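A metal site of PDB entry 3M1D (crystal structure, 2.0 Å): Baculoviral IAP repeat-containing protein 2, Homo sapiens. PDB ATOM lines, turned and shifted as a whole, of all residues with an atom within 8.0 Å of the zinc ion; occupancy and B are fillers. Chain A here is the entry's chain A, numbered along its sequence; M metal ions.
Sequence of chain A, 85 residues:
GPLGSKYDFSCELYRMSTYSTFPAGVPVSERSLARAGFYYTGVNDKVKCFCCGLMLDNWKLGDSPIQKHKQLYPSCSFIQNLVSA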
ATOM      1  N   ALA A  36     -30.836   0.878  15.037  1.00  0.00           N
ATOM      2  CA  ALA A  36     -29.509   0.696  15.650  1.00  0.00           C
ATOM      3  C   ALA A  36     -29.000   1.972  16.324  1.00  0.00           C
ATOM      4  O   ALA A  36     -27.879   2.010  16.815  1.00  0.00           O
ATOM      5  CB  ALA A  36     -28.510   0.180  14.620  1.00  0.00           C
ATOM      6  N   GLY A  37     -29.838   3.000  16.352  1.00  0.00           N
ATOM      7  CA  GLY A  37     -29.525   4.242  17.053  1.00  0.00           C
ATOM      8  C   GLY A  37     -28.989   5.335  16.145  1.00  0.00           C
ATOM      9  O   GLY A  37     -28.625   6.401  16.621  1.00  0.00           O
ATOM     10  N   PHE A  38     -28.944   5.070  14.849  1.00  0.00           N
ATOM     11  CA  PHE A  38     -28.305   6.020  13.944  1.00  0.00           C
ATOM     12  C   PHE A  38     -29.279   6.976  13.280  1.00  0.00           C
ATOM     13  O   PHE A  38     -30.330   6.563  12.814  1.00  0.00           O
ATOM     14  CB  PHE A  38     -27.524   5.272  12.856  1.00  0.00           C
ATOM     15  CG  PHE A  38     -26.344   4.503  13.382  1.00  0.00           C
ATOM     16  CD1 PHE A  38     -25.206   5.159  13.808  1.00  0.00           C
ATOM     17  CD2 PHE A  38     -26.372   3.121  13.438  1.00  0.00           C
ATOM     18  CE1 PHE A  38     -24.107   4.460  14.284  1.00  0.00           C
ATOM     19  CE2 PHE A  38     -25.278   2.401  13.905  1.00  0.00           C
ATOM     20  CZ  PHE A  38     -24.135   3.078  14.339  1.00  0.00           C
ATOM     21  N   LYS A  48     -25.006   8.789  12.291  1.00  0.00           N
ATOM     22  CA  LYS A  48     -24.380   9.066  13.570  1.00  0.00           C
ATOM     23  C   LYS A  48     -25.280   8.527  14.688  1.00  0.00           C
ATOM     24  O   LYS A  48     -26.493   8.655  14.621  1.00  0.00           O
ATOM     25  CB  LYS A  48     -24.185  10.595  13.684  1.00  0.00           C
ATOM     26  CG  LYS A  48     -23.347  11.100  14.853  1.00  0.00           C
ATOM     27  CD  LYS A  48     -23.032  12.596  14.638  1.00  0.00           C
ATOM     28  CE  LYS A  48     -22.484  13.262  15.899  1.00  0.00           C
ATOM     29  NZ  LYS A  48     -22.672  14.754  15.847  1.00  0.00           N
ATOM     30  N   CYS A  49     -24.682   7.900  15.702  1.00  0.00           N
ATOM     31  CA  CYS A  49     -25.490   7.413  16.827  1.00  0.00           C
ATOM     32  C   CYS A  49     -25.936   8.573  17.687  1.00  0.00           C
ATOM     33  O   CYS A  49     -25.140   9.437  18.061  1.00  0.00           O
ATOM     34  CB  CYS A  49     -24.710   6.416  17.685  1.00  0.00           C
ATOM     35  SG  CYS A  49     -25.671   5.847  19.114  1.00  0.00           S
ATOM     36  N   PHE A  50     -27.230   8.606  17.996  1.00  0.00           N
ATOM     37  CA  PHE A  50     -27.798   9.650  18.830  1.00  0.00           C
ATOM     38  C   PHE A  50     -27.251   9.577  20.259  1.00  0.00           C
ATOM     39  O   PHE A  50     -27.271  10.578  20.978  1.00  0.00           O
ATOM     40  CB  PHE A  50     -29.342   9.560  18.841  1.00  0.00           C
ATOM     41  CG  PHE A  50     -29.895   8.494  19.762  1.00  0.00           C
ATOM     42  CD1 PHE A  50     -30.785   8.831  20.770  1.00  0.00           C
ATOM     43  CD2 PHE A  50     -29.552   7.162  19.594  1.00  0.00           C
ATOM     44  CE1 PHE A  50     -31.305   7.858  21.615  1.00  0.00           C
ATOM     45  CE2 PHE A  50     -30.079   6.180  20.418  1.00  0.00           C
ATOM     46  CZ  PHE A  50     -30.956   6.533  21.437  1.00  0.00           C
ATOM     47  N   CYS A  51     -26.741   8.417  20.653  1.00  0.00           N
ATOM     48  CA  CYS A  51     -26.272   8.233  22.024  1.00  0.00           C
ATOM     49  C   CYS A  51     -24.785   8.510  22.203  1.00  0.00           C
ATOM     50  O   CYS A  51     -24.395   9.242  23.114  1.00  0.00           O
ATOM     51  CB  CYS A  51     -26.577   6.818  22.523  1.00  0.00           C
ATOM     52  SG  CYS A  51     -25.996   6.509  24.220  1.00  0.00           S
ATOM     53  N   CYS A  52     -23.957   7.935  21.345  1.00  0.00           N
ATOM     54  CA  CYS A  52     -22.511   8.035  21.526  1.00  0.00           C
ATOM     55  C   CYS A  52     -21.804   8.826  20.430  1.00  0.00           C
ATOM     56  O   CYS A  52     -20.616   9.113  20.552  1.00  0.00           O
ATOM     57  CB  CYS A  52     -21.875   6.638  21.629  1.00  0.00           C
ATOM     58  SG  CYS A  52     -21.902   5.677  20.050  1.00  0.00           S
ATOM     59  N   GLY A  53     -22.519   9.174  19.370  1.00  0.00           N
ATOM     60  CA  GLY A  53     -21.893   9.952  18.307  1.00  0.00           C
ATOM     61  C   GLY A  53     -21.013   9.153  17.345  1.00  0.00           C
ATOM     62  O   GLY A  53     -20.335   9.729  16.498  1.00  0.00           O
ATOM     63  N   LEU A  54     -20.993   7.830  17.457  1.00  0.00           N
ATOM     64  CA  LEU A  54     -20.257   7.018  16.481  1.00  0.00           C
ATOM     65  C   LEU A  54     -20.750   7.348  15.064  1.00  0.00           C
ATOM     66  O   LEU A  54     -21.948   7.401  14.823  1.00  0.00           O
ATOM     67  CB  LEU A  54     -20.435   5.529  16.762  1.00  0.00           C
ATOM     68  CG  LEU A  54     -19.853   4.537  15.759  1.00  0.00           C
ATOM     69  CD1 LEU A  54     -18.327   4.520  15.830  1.00  0.00           C
ATOM     70  CD2 LEU A  54     -20.427   3.160  16.059  1.00  0.00           C
ATOM     71  N   MET A  55     -19.814   7.551  14.134  1.00  0.00           N
ATOM     72  CA  MET A  55     -20.149   7.932  12.761  1.00  0.00           C
ATOM     73  C   MET A  55     -19.724   6.869  11.758  1.00  0.00           C
ATOM     74  O   MET A  55     -18.578   6.413  11.777  1.00  0.00           O
ATOM     75  CB  MET A  55     -19.491   9.277  12.403  1.00  0.00           C
ATOM     76  CG  MET A  55     -20.061  10.448  13.209  1.00  0.00           C
ATOM     77  SD  MET A  55     -19.290  12.016  12.769  1.00  0.00           S
ATOM     78  CE  MET A  55     -20.270  12.426  11.342  1.00  0.00           C
ATOM     79  N   HIS A  69     -22.026  -1.261  15.229  1.00  0.00           N
ATOM     80  CA  HIS A  69     -22.163  -0.392  16.403  1.00  0.00           C
ATOM     81  C   HIS A  69     -21.557  -1.046  17.652  1.00  0.00           C
ATOM     82  O   HIS A  69     -20.744  -0.421  18.352  1.00  0.00           O
ATOM     83  CB  HIS A  69     -23.642  -0.115  16.624  1.00  0.00           C
ATOM     84  CG  HIS A  69     -23.909   1.097  17.460  1.00  0.00           C
ATOM     85  ND1 HIS A  69     -25.140   1.733  17.459  1.00  0.00           N
ATOM     86  CD2 HIS A  69     -23.125   1.780  18.323  1.00  0.00           C
ATOM     87  CE1 HIS A  69     -25.092   2.767  18.285  1.00  0.00           C
ATOM     88  NE2 HIS A  69     -23.877   2.825  18.818  1.00  0.00           N
ATOM     89  N   LYS A  70     -21.977  -2.277  17.942  1.00  0.00           N
ATOM     90  CA  LYS A  70     -21.466  -3.049  19.077  1.00  0.00           C
ATOM     91  C   LYS A  70     -19.963  -3.233  19.028  1.00  0.00           C
ATOM     92  O   LYS A  70     -19.292  -3.173  20.055  1.00  0.00           O
ATOM     93  CB  LYS A  70     -22.090  -4.462  19.098  1.00  0.00           C
ATOM     94  CG  LYS A  70     -23.414  -4.574  19.814  1.00  0.00           C
ATOM     95  CD  LYS A  70     -24.197  -5.797  19.343  1.00  0.00           C
ATOM     96  CE  LYS A  70     -23.390  -7.096  19.467  1.00  0.00           C
ATOM     97  NZ  LYS A  70     -24.244  -8.324  19.333  1.00  0.00           N
ATOM     98  N   TYR A  73     -18.001   0.674  19.008  1.00  0.00           N
ATOM     99  CA  TYR A  73     -18.179   1.463  20.224  1.00  0.00           C
ATOM    100  C   TYR A  73     -19.086   0.796  21.252  1.00  0.00           C
ATOM    101  O   TYR A  73     -20.224   1.215  21.458  1.00  0.00           O
ATOM    102  CB  TYR A  73     -18.674   2.875  19.895  1.00  0.00           C
ATOM    103  CG  TYR A  73     -18.142   3.888  20.879  1.00  0.00           C
ATOM    104  CD1 TYR A  73     -16.813   4.309  20.801  1.00  0.00           C
ATOM    105  CD2 TYR A  73     -18.928   4.379  21.904  1.00  0.00           C
ATOM    106  CE1 TYR A  73     -16.304   5.221  21.709  1.00  0.00           C
ATOM    107  CE2 TYR A  73     -18.425   5.283  22.822  1.00  0.00           C
ATOM    108  CZ  TYR A  73     -17.104   5.696  22.723  1.00  0.00           C
ATOM    109  OH  TYR A  73     -16.610   6.592  23.629  1.00  0.00           O
ATOM    110  N   PRO A  74     -18.564  -0.253  21.916  1.00  0.00           N
ATOM    111  CA  PRO A  74     -19.317  -1.085  22.860  1.00  0.00           C
ATOM    112  C   PRO A  74     -19.784  -0.319  24.098  1.00  0.00           C
ATOM    113  O   PRO A  74     -20.717  -0.777  24.761  1.00  0.00           O
ATOM    114  CB  PRO A  74     -18.293  -2.153  23.301  1.00  0.00           C
ATOM    115  CG  PRO A  74     -17.067  -1.945  22.475  1.00  0.00           C
ATOM    116  CD  PRO A  74     -17.128  -0.582  21.889  1.00  0.00           C
ATOM    117  N   SER A  75     -19.161   0.818  24.414  1.00  0.00           N
ATOM    118  CA  SER A  75     -19.473   1.529  25.657  1.00  0.00           C
ATOM    119  C   SER A  75     -20.739   2.388  25.555  1.00  0.00           C
ATOM    120  O   SER A  75     -21.198   2.941  26.553  1.00  0.00           O
ATOM    121  CB  SER A  75     -18.279   2.359  26.137  1.00  0.00           C
ATOM    122  OG  SER A  75     -18.000   3.429  25.250  1.00  0.00           O
ATOM    123  N   CYS A  76     -21.291   2.481  24.351  1.00  0.00           N
ATOM    124  CA  CYS A  76     -22.557   3.176  24.135  1.00  0.00           C
ATOM    125  C   CYS A  76     -23.663   2.520  24.956  1.00  0.00           C
ATOM    126  O   CYS A  76     -23.984   1.351  24.732  1.00  0.00           O
ATOM    127  CB  CYS A  76     -22.927   3.140  22.651  1.00  0.00           C
ATOM    128  SG  CYS A  76     -24.552   3.842  22.280  1.00  0.00           S
ATOM    129  N   SER A  77     -24.256   3.278  25.871  1.00  0.00           N
ATOM    130  CA  SER A  77     -25.343   2.754  26.711  1.00  0.00           C
ATOM    131  C   SER A  77     -26.520   2.288  25.866  1.00  0.00           C
ATOM    132  O   SER A  77     -27.169   1.290  26.202  1.00  0.00           O
ATOM    133  CB  SER A  77     -25.839   3.820  27.695  1.00  0.00           C
ATOM    134  OG  SER A  77     -24.811   4.214  28.584  1.00  0.00           O
ATOM    135  N   PHE A  78     -26.827   2.999  24.790  1.00  0.00           N
ATOM    136  CA  PHE A  78     -27.948   2.588  23.973  1.00  0.00           C
ATOM    137  C   PHE A  78     -27.697   1.209  23.362  1.00  0.00           C
ATOM    138  O   PHE A  78     -28.497   0.282  23.546  1.00  0.00           O
ATOM    139  CB  PHE A  78     -28.252   3.595  22.861  1.00  0.00           C
ATOM    140  CG  PHE A  78     -29.264   3.096  21.875  1.00  0.00           C
ATOM    141  CD1 PHE A  78     -30.619   3.170  22.143  1.00  0.00           C
ATOM    142  CD2 PHE A  78     -28.853   2.521  20.681  1.00  0.00           C
ATOM    143  CE1 PHE A  78     -31.561   2.691  21.235  1.00  0.00           C
ATOM    144  CE2 PHE A  78     -29.792   2.041  19.764  1.00  0.00           C
ATOM    145  CZ  PHE A  78     -31.148   2.127  20.050  1.00  0.00           C
ATOM    146  N   ILE A  79     -26.590   1.049  22.647  1.00  0.00           N
ATOM    147  CA  ILE A  79     -26.313  -0.223  21.997  1.00  0.00           C
ATOM    148  C   ILE A  79     -26.232  -1.376  23.019  1.00  0.00           C
ATOM    149  O   ILE A  79     -26.609  -2.495  22.712  1.00  0.00           O
ATOM    150  CB  ILE A  79     -25.054  -0.190  21.077  1.00  0.00           C
ATOM    151  CG1 ILE A  79     -25.184  -1.236  19.961  1.00  0.00           C
ATOM    152  CG2 ILE A  79     -23.771  -0.434  21.874  1.00  0.00           C
ATOM    153  CD1 ILE A  79     -26.405  -1.029  19.060  1.00  0.00           C
ATOM    154  N   GLN A  80     -25.771  -1.084  24.244  1.00  0.00           N
ATOM    155  CA  GLN A  80     -25.707  -2.102  25.296  1.00  0.00           C
ATOM    156  C   GLN A  80     -27.101  -2.529  25.732  1.00  0.00           C
ATOM    157  O   GLN A  80     -27.361  -3.715  25.942  1.00  0.00           O
ATOM    158  CB  GLN A  80     -24.938  -1.591  26.519  1.00  0.00           C
ATOM    159  CG  GLN A  80     -23.432  -1.535  26.378  1.00  0.00           C
ATOM    160  CD  GLN A  80     -22.781  -0.844  27.580  1.00  0.00           C
ATOM    161  OE1 GLN A  80     -21.556  -0.731  27.671  1.00  0.00           O
ATOM    162  NE2 GLN A  80     -23.613  -0.383  28.503  1.00  0.00           N
HETATM  163 ZN    ZN M   1     -23.962   4.595  20.139  1.00  0.00          ZN
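Four residues have an atom within 4 Å of the zinc ion: Cys 49, Cys 52, His 69 and Cys 76.
The zinc ion is bound by NE2 of His 69 (2.2 Å).
SG of Cys 52 binds the zinc ion (2.3 Å).
The zinc ion is bound by SG of Cys 76 (2.3 Å).
The zinc ion is bound by the side-chain sulfur (SG) of Cys 49 (2.4 Å).
The zinc ion has four donor atoms within binding distance.
A ring nitrogen (ND1) of His 69 sits at hydrogen-bond distance from the backbone carbonyl oxygen of Ala 36 (2.8 Å).
SG of Cys 52 sits close to N of Leu 54 (3.5 Å).
The side-chain sulfur (SG) of Cys 51 sits close to the side-chain sulfur (SG) of Cys 76, 3.6 Å away.
SG of Cys 76 lies close to N of Ile 79.
N of Phe 78 sits close to SG of Cys 76 (3.5 Å).
SG of Cys 49 lies close to N of Cys 51 (3.2 Å).
O of Leu 54 is in hydrogen-bond range of N of Cys 49 (2.9 Å).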
